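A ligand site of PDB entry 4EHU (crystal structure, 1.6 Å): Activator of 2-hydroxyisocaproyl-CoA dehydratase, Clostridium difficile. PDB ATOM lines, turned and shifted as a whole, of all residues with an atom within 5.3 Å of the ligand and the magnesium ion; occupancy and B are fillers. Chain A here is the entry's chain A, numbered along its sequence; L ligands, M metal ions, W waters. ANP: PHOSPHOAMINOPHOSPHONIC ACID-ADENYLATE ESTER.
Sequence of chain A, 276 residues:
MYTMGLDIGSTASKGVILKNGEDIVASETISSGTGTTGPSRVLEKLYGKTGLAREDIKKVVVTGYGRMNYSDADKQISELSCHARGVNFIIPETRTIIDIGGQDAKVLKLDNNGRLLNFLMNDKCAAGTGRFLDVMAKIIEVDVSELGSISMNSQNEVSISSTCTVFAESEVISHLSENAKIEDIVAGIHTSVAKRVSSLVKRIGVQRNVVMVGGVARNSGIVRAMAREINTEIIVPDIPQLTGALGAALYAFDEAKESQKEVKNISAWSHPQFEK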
ATOM      1  N   ASP A   7      23.664  25.176 -14.487  1.00  0.00           N
ATOM      2  CA  ASP A   7      24.306  25.420 -15.774  1.00  0.00           C
ATOM      3  C   ASP A   7      23.466  26.465 -16.507  1.00  0.00           C
ATOM      4  O   ASP A   7      22.384  26.170 -16.992  1.00  0.00           O
ATOM      5  CB  ASP A   7      24.429  24.102 -16.558  1.00  0.00           C
ATOM      6  CG  ASP A   7      24.939  24.284 -18.002  1.00  0.00           C
ATOM      7  OD1 ASP A   7      25.241  25.412 -18.443  1.00  0.00           O
ATOM      8  OD2 ASP A   7      25.022  23.273 -18.707  1.00  0.00           O
ATOM      9  N   GLY A   9      23.187  28.496 -19.523  1.00  0.00           N
ATOM     10  CA  GLY A   9      23.746  28.655 -20.849  1.00  0.00           C
ATOM     11  C   GLY A   9      23.121  29.818 -21.587  1.00  0.00           C
ATOM     12  O   GLY A   9      22.367  30.594 -21.004  1.00  0.00           O
ATOM     13  N   SER A  10      23.420  29.916 -22.865  1.00  0.00           N
ATOM     14  CA  SER A  10      22.881  30.980 -23.704  1.00  0.00           C
ATOM     15  C   SER A  10      21.367  30.899 -23.806  1.00  0.00           C
ATOM     16  O   SER A  10      20.692  31.899 -24.027  1.00  0.00           O
ATOM     17  CB  SER A  10      23.489  30.865 -25.098  1.00  0.00           C
ATOM     18  OG  SER A  10      23.032  29.722 -25.795  1.00  0.00           O
ATOM     19  N   THR A  11      20.843  29.690 -23.623  1.00  0.00           N
ATOM     20  CA  THR A  11      19.521  29.360 -24.137  1.00  0.00           C
ATOM     21  C   THR A  11      18.618  28.743 -23.095  1.00  0.00           C
ATOM     22  O   THR A  11      17.424  29.017 -23.056  1.00  0.00           O
ATOM     23  CB  THR A  11      19.655  28.371 -25.313  1.00  0.00           C
ATOM     24  OG1 THR A  11      20.445  28.975 -26.347  1.00  0.00           O
ATOM     25  CG2 THR A  11      18.281  27.989 -25.866  1.00  0.00           C
ATOM     26  N   ALA A  12      19.200  27.912 -22.227  1.00  0.00           N
ATOM     27  CA  ALA A  12      18.418  27.283 -21.181  1.00  0.00           C
ATOM     28  C   ALA A  12      19.178  27.219 -19.871  1.00  0.00           C
ATOM     29  O   ALA A  12      20.411  27.162 -19.876  1.00  0.00           O
ATOM     30  CB  ALA A  12      18.000  25.883 -21.600  1.00  0.00           C
ATOM     31  N   LYS A  14      19.796  25.016 -16.467  1.00  0.00           N
ATOM     32  CA  LYS A  14      19.688  23.628 -16.007  1.00  0.00           C
ATOM     33  C   LYS A  14      20.166  23.514 -14.581  1.00  0.00           C
ATOM     34  O   LYS A  14      21.148  24.156 -14.192  1.00  0.00           O
ATOM     35  CB  LYS A  14      20.531  22.715 -16.895  1.00  0.00           C
ATOM     36  CG  LYS A  14      19.939  22.440 -18.277  1.00  0.00           C
ATOM     37  CD  LYS A  14      20.117  23.628 -19.258  1.00  0.00           C
ATOM     38  CE  LYS A  14      21.580  23.820 -19.667  1.00  0.00           C
ATOM     39  NZ  LYS A  14      21.766  24.811 -20.782  1.00  0.00           N
ATOM     40  N   TYR A  65      27.743  29.870 -19.757  1.00  0.00           N
ATOM     41  CA  TYR A  65      27.950  31.223 -20.233  1.00  0.00           C
ATOM     42  C   TYR A  65      27.601  32.255 -19.185  1.00  0.00           C
ATOM     43  O   TYR A  65      28.278  33.273 -19.058  1.00  0.00           O
ATOM     44  CB  TYR A  65      27.091  31.430 -21.478  1.00  0.00           C
ATOM     45  CG  TYR A  65      27.223  32.795 -22.096  1.00  0.00           C
ATOM     46  CD1 TYR A  65      28.350  33.135 -22.828  1.00  0.00           C
ATOM     47  CD2 TYR A  65      26.200  33.717 -21.977  1.00  0.00           C
ATOM     48  CE1 TYR A  65      28.457  34.410 -23.414  1.00  0.00           C
ATOM     49  CE2 TYR A  65      26.301  34.973 -22.548  1.00  0.00           C
ATOM     50  CZ  TYR A  65      27.428  35.310 -23.271  1.00  0.00           C
ATOM     51  OH  TYR A  65      27.511  36.557 -23.834  1.00  0.00           O
ATOM     52  N   GLU A  79      32.432  25.272 -18.089  1.00  0.00           N
ATOM     53  CA  GLU A  79      31.508  24.253 -18.594  1.00  0.00           C
ATOM     54  C   GLU A  79      32.240  23.122 -19.314  1.00  0.00           C
ATOM     55  O   GLU A  79      31.676  22.037 -19.478  1.00  0.00           O
ATOM     56  CB  GLU A  79      30.423  24.853 -19.481  1.00  0.00           C
ATOM     57  CG  GLU A  79      30.910  25.291 -20.844  1.00  0.00           C
ATOM     58  CD  GLU A  79      30.035  26.396 -21.437  1.00  0.00           C
ATOM     59  OE1 GLU A  79      29.357  26.138 -22.461  1.00  0.00           O
ATOM     60  OE2 GLU A  79      30.072  27.542 -20.910  1.00  0.00           O
ATOM     61  N   HIS A  83      30.920  19.606 -18.092  1.00  0.00           N
ATOM     62  CA  HIS A  83      30.382  18.565 -18.964  1.00  0.00           C
ATOM     63  C   HIS A  83      31.240  17.306 -18.925  1.00  0.00           C
ATOM     64  O   HIS A  83      30.723  16.215 -18.901  1.00  0.00           O
ATOM     65  CB  HIS A  83      30.247  19.045 -20.414  1.00  0.00           C
ATOM     66  CG  HIS A  83      29.014  19.855 -20.670  1.00  0.00           C
ATOM     67  ND1 HIS A  83      27.746  19.319 -20.601  1.00  0.00           N
ATOM     68  CD2 HIS A  83      28.866  21.157 -21.039  1.00  0.00           C
ATOM     69  CE1 HIS A  83      26.866  20.259 -20.903  1.00  0.00           C
ATOM     70  NE2 HIS A  83      27.513  21.380 -21.152  1.00  0.00           N
ATOM     71  N   ASP A  99      29.333  18.645 -27.371  1.00  0.00           N
ATOM     72  CA  ASP A  99      28.308  19.406 -26.692  1.00  0.00           C
ATOM     73  C   ASP A  99      27.698  20.383 -27.678  1.00  0.00           C
ATOM     74  O   ASP A  99      28.296  21.392 -28.009  1.00  0.00           O
ATOM     75  CB  ASP A  99      28.931  20.173 -25.506  1.00  0.00           C
ATOM     76  CG  ASP A  99      28.067  21.320 -25.001  1.00  0.00           C
ATOM     77  OD1 ASP A  99      26.827  21.193 -25.030  1.00  0.00           O
ATOM     78  OD2 ASP A  99      28.641  22.352 -24.558  1.00  0.00           O
ATOM     79  N   ILE A 100      26.490  20.085 -28.162  1.00  0.00           N
ATOM     80  CA  ILE A 100      25.837  21.033 -29.051  1.00  0.00           C
ATOM     81  C   ILE A 100      24.782  21.789 -28.267  1.00  0.00           C
ATOM     82  O   ILE A 100      23.792  21.209 -27.848  1.00  0.00           O
ATOM     83  CB  ILE A 100      25.193  20.336 -30.264  1.00  0.00           C
ATOM     84  CG1 ILE A 100      26.236  19.475 -30.990  1.00  0.00           C
ATOM     85  CG2 ILE A 100      24.653  21.431 -31.188  1.00  0.00           C
ATOM     86  CD1 ILE A 100      25.647  18.620 -32.208  1.00  0.00           C
ATOM     87  N   GLY A 101      25.043  23.086 -28.041  1.00  0.00           N
ATOM     88  CA  GLY A 101      24.130  23.929 -27.283  1.00  0.00           C
ATOM     89  C   GLY A 101      23.389  24.896 -28.194  1.00  0.00           C
ATOM     90  O   GLY A 101      23.361  24.723 -29.415  1.00  0.00           O
ATOM     91  N   GLY A 102      22.801  25.918 -27.581  1.00  0.00           N
ATOM     92  CA  GLY A 102      22.020  26.909 -28.292  1.00  0.00           C
ATOM     93  C   GLY A 102      22.818  27.978 -29.010  1.00  0.00           C
ATOM     94  O   GLY A 102      22.305  28.596 -29.935  1.00  0.00           O
ATOM     95  N   GLN A 103      24.062  28.226 -28.598  1.00  0.00           N
ATOM     96  CA  GLN A 103      24.862  29.225 -29.309  1.00  0.00           C
ATOM     97  C   GLN A 103      26.241  28.752 -29.753  1.00  0.00           C
ATOM     98  O   GLN A 103      26.886  29.407 -30.585  1.00  0.00           O
ATOM     99  CB  GLN A 103      24.996  30.528 -28.493  1.00  0.00           C
ATOM    100  CG  GLN A 103      26.029  30.471 -27.378  1.00  0.00           C
ATOM    101  CD  GLN A 103      26.251  31.850 -26.739  1.00  0.00           C
ATOM    102  OE1 GLN A 103      25.588  32.825 -27.097  1.00  0.00           O
ATOM    103  NE2 GLN A 103      27.192  31.927 -25.808  1.00  0.00           N
ATOM    104  N   ASP A 104      26.715  27.629 -29.221  1.00  0.00           N
ATOM    105  CA  ASP A 104      27.972  27.097 -29.727  1.00  0.00           C
ATOM    106  C   ASP A 104      28.012  25.580 -29.656  1.00  0.00           C
ATOM    107  O   ASP A 104      27.190  24.965 -28.997  1.00  0.00           O
ATOM    108  CB  ASP A 104      29.216  27.734 -29.079  1.00  0.00           C
ATOM    109  CG  ASP A 104      29.372  27.424 -27.579  1.00  0.00           C
ATOM    110  OD1 ASP A 104      29.440  26.232 -27.222  1.00  0.00           O
ATOM    111  OD2 ASP A 104      29.475  28.392 -26.777  1.00  0.00           O
ATOM    112  N   LYS A 106      30.755  22.492 -28.954  1.00  0.00           N
ATOM    113  CA  LYS A 106      32.060  22.244 -28.392  1.00  0.00           C
ATOM    114  C   LYS A 106      32.431  20.801 -28.578  1.00  0.00           C
ATOM    115  O   LYS A 106      31.602  19.908 -28.370  1.00  0.00           O
ATOM    116  CB  LYS A 106      32.033  22.553 -26.889  1.00  0.00           C
ATOM    117  CG  LYS A 106      31.827  24.031 -26.566  1.00  0.00           C
ATOM    118  CD  LYS A 106      31.760  24.206 -25.046  1.00  0.00           C
ATOM    119  CE  LYS A 106      32.087  25.662 -24.658  1.00  0.00           C
ATOM    120  NZ  LYS A 106      30.942  26.585 -24.918  1.00  0.00           N
ATOM    121  N   GLY A 130      22.136  24.758 -31.904  1.00  0.00           N
ATOM    122  CA  GLY A 130      20.718  24.778 -31.621  1.00  0.00           C
ATOM    123  C   GLY A 130      19.986  25.966 -32.231  1.00  0.00           C
ATOM    124  O   GLY A 130      18.808  25.867 -32.548  1.00  0.00           O
ATOM    125  N   ARG A 131      20.671  27.096 -32.371  1.00  0.00           N
ATOM    126  CA  ARG A 131      20.057  28.272 -32.945  1.00  0.00           C
ATOM    127  C   ARG A 131      19.597  27.993 -34.364  1.00  0.00           C
ATOM    128  O   ARG A 131      18.517  28.405 -34.766  1.00  0.00           O
ATOM    129  CB  ARG A 131      21.053  29.426 -32.978  1.00  0.00           C
ATOM    130  CG  ARG A 131      20.423  30.728 -33.421  1.00  0.00           C
ATOM    131  CD  ARG A 131      19.227  31.066 -32.541  1.00  0.00           C
ATOM    132  NE  ARG A 131      18.706  32.381 -32.843  1.00  0.00           N
ATOM    133  CZ  ARG A 131      19.084  33.497 -32.217  1.00  0.00           C
ATOM    134  NH1 ARG A 131      19.966  33.452 -31.233  1.00  0.00           N
ATOM    135  NH2 ARG A 131      18.561  34.652 -32.578  1.00  0.00           N
ATOM    136  N   LEU A 133      18.717  25.132 -35.605  1.00  0.00           N
ATOM    137  CA  LEU A 133      17.536  24.258 -35.542  1.00  0.00           C
ATOM    138  C   LEU A 133      16.330  25.049 -35.072  1.00  0.00           C
ATOM    139  O   LEU A 133      15.239  24.849 -35.577  1.00  0.00           O
ATOM    140  CB  LEU A 133      17.806  23.077 -34.601  1.00  0.00           C
ATOM    141  CG  LEU A 133      18.903  22.165 -35.165  1.00  0.00           C
ATOM    142  CD1 LEU A 133      19.460  21.222 -34.081  1.00  0.00           C
ATOM    143  CD2 LEU A 133      18.356  21.331 -36.334  1.00  0.00           C
ATOM    144  N   ASP A 134      16.513  25.960 -34.122  1.00  0.00           N
ATOM    145  CA  ASP A 134      15.379  26.711 -33.594  1.00  0.00           C
ATOM    146  C   ASP A 134      14.827  27.593 -34.721  1.00  0.00           C
ATOM    147  O   ASP A 134      13.613  27.711 -34.896  1.00  0.00           O
ATOM    148  CB  ASP A 134      15.791  27.558 -32.385  1.00  0.00           C
ATOM    149  CG  ASP A 134      16.286  26.703 -31.204  1.00  0.00           C
ATOM    150  OD1 ASP A 134      16.026  25.480 -31.170  1.00  0.00           O
ATOM    151  OD2 ASP A 134      16.943  27.274 -30.312  1.00  0.00           O
ATOM    152  N   VAL A 144      10.738  22.075 -31.967  1.00  0.00           N
ATOM    153  CA  VAL A 144      12.068  21.491 -32.068  1.00  0.00           C
ATOM    154  C   VAL A 144      12.063  20.077 -31.492  1.00  0.00           C
ATOM    155  O   VAL A 144      12.856  19.232 -31.908  1.00  0.00           O
ATOM    156  CB  VAL A 144      13.154  22.350 -31.358  1.00  0.00           C
ATOM    157  CG1 VAL A 144      13.279  23.694 -32.048  1.00  0.00           C
ATOM    158  CG2 VAL A 144      12.836  22.525 -29.886  1.00  0.00           C
ATOM    159  N   SER A 145      11.164  19.817 -30.555  1.00  0.00           N
ATOM    160  CA  SER A 145      11.078  18.495 -29.912  1.00  0.00           C
ATOM    161  C   SER A 145      10.532  17.400 -30.835  1.00  0.00           C
ATOM    162  O   SER A 145      10.631  16.219 -30.507  1.00  0.00           O
ATOM    163  CB  SER A 145      10.224  18.559 -28.638  1.00  0.00           C
ATOM    164  OG  SER A 145       8.859  18.787 -28.961  1.00  0.00           O
ATOM    165  N   GLY A 214      24.222  18.214 -24.395  1.00  0.00           N
ATOM    166  CA  GLY A 214      23.579  19.451 -24.797  1.00  0.00           C
ATOM    167  C   GLY A 214      22.133  19.193 -25.177  1.00  0.00           C
ATOM    168  O   GLY A 214      21.720  18.031 -25.404  1.00  0.00           O
ATOM    169  N   GLY A 215      21.375  20.277 -25.281  1.00  0.00           N
ATOM    170  CA  GLY A 215      19.951  20.173 -25.563  1.00  0.00           C
ATOM    171  C   GLY A 215      19.709  19.598 -26.965  1.00  0.00           C
ATOM    172  O   GLY A 215      18.718  18.901 -27.183  1.00  0.00           O
ATOM    173  N   VAL A 216      20.620  19.885 -27.902  1.00  0.00           N
ATOM    174  CA  VAL A 216      20.461  19.399 -29.274  1.00  0.00           C
ATOM    175  C   VAL A 216      20.617  17.893 -29.329  1.00  0.00           C
ATOM    176  O   VAL A 216      20.095  17.246 -30.241  1.00  0.00           O
ATOM    177  CB  VAL A 216      21.442  20.102 -30.223  1.00  0.00           C
ATOM    178  CG1 VAL A 216      21.387  19.516 -31.644  1.00  0.00           C
ATOM    179  CG2 VAL A 216      21.121  21.588 -30.256  1.00  0.00           C
ATOM    180  N   ARG A 218      19.106  15.922 -27.517  1.00  0.00           N
ATOM    181  CA  ARG A 218      17.763  15.386 -27.340  1.00  0.00           C
ATOM    182  C   ARG A 218      17.070  15.115 -28.686  1.00  0.00           C
ATOM    183  O   ARG A 218      16.043  14.437 -28.715  1.00  0.00           O
ATOM    184  CB  ARG A 218      16.902  16.336 -26.512  1.00  0.00           C
ATOM    185  CG  ARG A 218      17.430  16.545 -25.109  1.00  0.00           C
ATOM    186  CD  ARG A 218      16.603  17.582 -24.389  1.00  0.00           C
ATOM    187  NE  ARG A 218      15.274  17.116 -24.049  1.00  0.00           N
ATOM    188  CZ  ARG A 218      14.361  17.887 -23.465  1.00  0.00           C
ATOM    189  NH1 ARG A 218      14.645  19.168 -23.203  1.00  0.00           N
ATOM    190  NH2 ARG A 218      13.171  17.399 -23.168  1.00  0.00           N
ATOM    191  N   ASN A 219      17.613  15.678 -29.771  1.00  0.00           N
ATOM    192  CA  ASN A 219      17.079  15.470 -31.120  1.00  0.00           C
ATOM    193  C   ASN A 219      17.702  14.216 -31.711  1.00  0.00           C
ATOM    194  O   ASN A 219      18.865  14.226 -32.094  1.00  0.00           O
ATOM    195  CB  ASN A 219      17.409  16.705 -31.980  1.00  0.00           C
ATOM    196  CG  ASN A 219      16.859  16.589 -33.381  1.00  0.00           C
ATOM    197  OD1 ASN A 219      16.709  15.491 -33.910  1.00  0.00           O
ATOM    198  ND2 ASN A 219      16.549  17.720 -33.977  1.00  0.00           N
ATOM    199  N   GLN A 241      20.998  17.088 -21.805  1.00  0.00           N
ATOM    200  CA  GLN A 241      20.997  18.535 -21.615  1.00  0.00           C
ATOM    201  C   GLN A 241      21.469  18.935 -20.207  1.00  0.00           C
ATOM    202  O   GLN A 241      21.775  20.094 -19.957  1.00  0.00           O
ATOM    203  CB  GLN A 241      19.586  19.091 -21.863  1.00  0.00           C
ATOM    204  CG  GLN A 241      19.535  20.612 -21.953  1.00  0.00           C
ATOM    205  CD  GLN A 241      18.184  21.091 -22.421  1.00  0.00           C
ATOM    206  OE1 GLN A 241      17.197  20.346 -22.412  1.00  0.00           O
ATOM    207  NE2 GLN A 241      18.131  22.350 -22.850  1.00  0.00           N
HETATM  208  PG  ANP L   1      25.385  27.156 -24.919  1.00  0.00           P
HETATM  209  O1G ANP L   1      25.773  28.425 -24.175  1.00  0.00           O
HETATM  210  O2G ANP L   1      26.002  25.951 -24.261  1.00  0.00           O
HETATM  211  O3G ANP L   1      25.670  27.224 -26.378  1.00  0.00           O
HETATM  212  PB  ANP L   1      22.796  26.169 -23.708  1.00  0.00           P
HETATM  213  O1B ANP L   1      21.719  26.995 -23.047  1.00  0.00           O
HETATM  214  O2B ANP L   1      23.673  25.329 -22.785  1.00  0.00           O
HETATM  215  N3B ANP L   1      23.680  27.188 -24.785  1.00  0.00           N
HETATM  216  PA  ANP L   1      21.403  23.685 -24.324  1.00  0.00           P
HETATM  217  O1A ANP L   1      20.534  23.875 -23.131  1.00  0.00           O
HETATM  218  O2A ANP L   1      22.543  22.692 -24.312  1.00  0.00           O
HETATM  219  O3A ANP L   1      22.064  25.114 -24.718  1.00  0.00           O
HETATM  220  O5' ANP L   1      20.551  23.406 -25.659  1.00  0.00           O
HETATM  221  C5' ANP L   1      19.612  24.383 -26.127  1.00  0.00           C
HETATM  222  C4' ANP L   1      18.845  23.784 -27.303  1.00  0.00           C
HETATM  223  O4' ANP L   1      18.577  22.382 -27.312  1.00  0.00           O
HETATM  224  C3' ANP L   1      17.916  24.556 -28.217  1.00  0.00           C
HETATM  225  O3' ANP L   1      18.647  25.502 -29.009  1.00  0.00           O
HETATM  226  C2' ANP L   1      17.238  23.438 -29.028  1.00  0.00           C
HETATM  227  O2' ANP L   1      17.693  23.387 -30.385  1.00  0.00           O
HETATM  228  C1' ANP L   1      17.602  22.121 -28.330  1.00  0.00           C
HETATM  229  N9  ANP L   1      16.471  21.495 -27.626  1.00  0.00           N
HETATM  230  C8  ANP L   1      15.909  21.883 -26.465  1.00  0.00           C
HETATM  231  N7  ANP L   1      14.933  21.030 -26.090  1.00  0.00           N
HETATM  232  C5  ANP L   1      14.866  20.067 -27.051  1.00  0.00           C
HETATM  233  C6  ANP L   1      14.074  18.863 -27.285  1.00  0.00           C
HETATM  234  N6  ANP L   1      13.097  18.533 -26.394  1.00  0.00           N
HETATM  235  N1  ANP L   1      14.337  18.126 -28.395  1.00  0.00           N
HETATM  236  C2  ANP L   1      15.292  18.451 -29.267  1.00  0.00           C
HETATM  237  N3  ANP L   1      16.054  19.551 -29.122  1.00  0.00           N
HETATM  238  C4  ANP L   1      15.896  20.366 -28.051  1.00  0.00           C
HETATM  239 MG    MG M   1      25.610  24.603 -22.727  1.00  0.00          MG
HETATM  240  O   HOH W   1      17.225  20.258 -31.732  1.00  0.00           O
HETATM  241  O   HOH W   2      27.597  23.968 -22.744  1.00  0.00           O
HETATM  242  O   HOH W   3      25.991  25.751 -20.985  1.00  0.00           O
HETATM  243  O   HOH W   4      11.542  20.212 -24.577  1.00  0.00           O
HETATM  244  O   HOH W   5      25.081  23.093 -21.270  1.00  0.00           O
HETATM  245  O   HOH W   6      27.224  28.018 -21.919  1.00  0.00           O
HETATM  246  O   HOH W   7      13.302  22.476 -24.303  1.00  0.00           O
HETATM  247  O   HOH W   8      13.507  15.633 -29.293  1.00  0.00           O
HETATM  248  O   HOH W   9      23.188  21.420 -21.935  1.00  0.00           O
HETATM  249  O   HOH W  10      11.712  16.058 -26.285  1.00  0.00           O
HETATM  250  O   HOH W  11      27.535  24.508 -26.034  1.00  0.00           O
HETATM  251  O   HOH W  12      28.262  29.407 -24.706  1.00  0.00           O
HETATM  252  O   HOH W  13      25.173  23.140 -24.199  1.00  0.00           O
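O of Ala 12 lies within hydrogen-bond range of NZ of Lys 14 (2.9 Å).
N of Gln 103 sits at hydrogen-bond distance from OG of Ser 10.
The backbone NH (N) of Asp 7 lies within hydrogen-bond range of the backbone carbonyl oxygen (O) of Lys 14, at 2.7 Å.
NH1 of Arg 218 sits at hydrogen-bond distance from OE1 of Gln 241, 2.9 Å away.
The side-chain carboxylate (OD1) of Asp 104 is in salt-bridge range of the side-chain amino group (NZ) of Lys 106 (2.8 Å).
The backbone carbonyl oxygen of Ile 100 is in hydrogen-bond range of the backbone NH of Val 216.
O of Gly 101 lies within hydrogen-bond range of N of Gly 130, at 2.8 Å.
OE2 of Glu 79 is in hydrogen-bond range of N of Tyr 65, 3.5 Å away.
Gly 9 touches the ligand (CA to O1B, 3.4 Å).
Glu 79 touches the ligand.
Gly 101 touches the ligand.
O of Val 144 touches C2 of the ligand, at 3.7 Å.
CA of Ser 145 touches N1 of the ligand (3.6 Å).
Gly 214 touches the ligand (CA to O2A, 3.4 Å).
Asn 219 touches the ligand.
Hydrophobic or aromatic side chains that line the ligand: Ala 12 and Val 216.
20 residues have an atom within 4 Å of the ligand: Gly 9, Ser 10, Thr 11, Ala 12, Lys 14, Glu 79, Gly 101, Gly 102, Gln 103, Asp 104, Gly 130, Asp 134, Val 144, Ser 145, Gly 214, Gly 215, Val 216, Arg 218, Asn 219 and Gln 241.
The nearest printed residue that does not touch the ligand is Ile 100 (4.03 Å).
The side-chain carboxylate of Asp 134 lies within hydrogen-bond range of an oxygen (O3') of the ligand, 2.8 Å away.
N of Ala 12 is in hydrogen-bond range of O1B of the ligand (2.8 Å).
The backbone NH (N) of Ser 10 lies within hydrogen-bond range of an oxygen (O1G) of the ligand, at 3.1 Å.
A nitrogen (N3B) of the ligand is in hydrogen-bond range of the side-chain hydroxyl of Ser 10.
NZ of Lys 14 lies within salt-bridge range of O1A of the ligand, at 2.8 Å.
The backbone NH of Gly 215 is in hydrogen-bond range of an oxygen (O2A) of the ligand.
NE2 of Gln 241 sits at hydrogen-bond distance from O1A of the ligand, at 2.9 Å.
An oxygen (O1B) of the ligand sits at hydrogen-bond distance from the backbone NH (N) of Thr 11 (2.9 Å).
O3G of the ligand lies within hydrogen-bond range of N of Gln 103.
The backbone NH (N) of Asp 104 sits at hydrogen-bond distance from an oxygen (O3G) of the ligand, at 3.1 Å.
The backbone NH of Gly 102 sits at hydrogen-bond distance from an oxygen (O3A) of the ligand (3.1 Å).
The guanidinium group (NH1) of Arg 218 sits at hydrogen-bond distance from a nitrogen (N7) of the ligand, 3.4 Å away.
N of Val 216 sits at hydrogen-bond distance from O4' of the ligand (3.3 Å).
The backbone carbonyl oxygen (O) of Gly 130 lies within hydrogen-bond range of an oxygen (O2') of the ligand, at 3.5 Å.
No residue comes within 4 Å of the magnesium ion.
The magnesium ion is bound by O2B of the ligand (2.1 Å), O2G of the ligand (2.1 Å), water W2 (2.1 Å), water W13 (2.1 Å), water W3 (2.1 Å) and water W5 (2.2 Å).
The magnesium ion has six donor atoms within binding distance.
Water W5 lies within hydrogen-bond range of the side-chain carboxylate (OD2) of Asp 7 (2.6 Å) and a ring nitrogen (NE2) of His 83 (3.0 Å).
Water W2 lies within hydrogen-bond range of OD2 of Asp 99, OE1 of Glu 79 and NE2 of His 83.
Water W6 lies within hydrogen-bond range of an oxygen (O1G) of the ligand (2.7 Å), the backbone NH (N) of Tyr 65 (2.9 Å) and the side-chain carboxylate (OE1) of Glu 79 (2.9 Å).
Water W11 lies within hydrogen-bond range of the side-chain carboxylate (OD1) of Asp 104 (2.8 Å), the side-chain carboxylate (OD2) of Asp 99 (2.8 Å) and an oxygen (O3G) of the ligand (3.3 Å).
Water W9 lies within hydrogen-bond range of O of Gln 241 (2.8 Å) and O2A of the ligand (2.8 Å).
Water W1 bridges a nitrogen (N3) of the ligand (2.9 Å) and the side-chain amide nitrogen of Asn 219 (3.5 Å).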
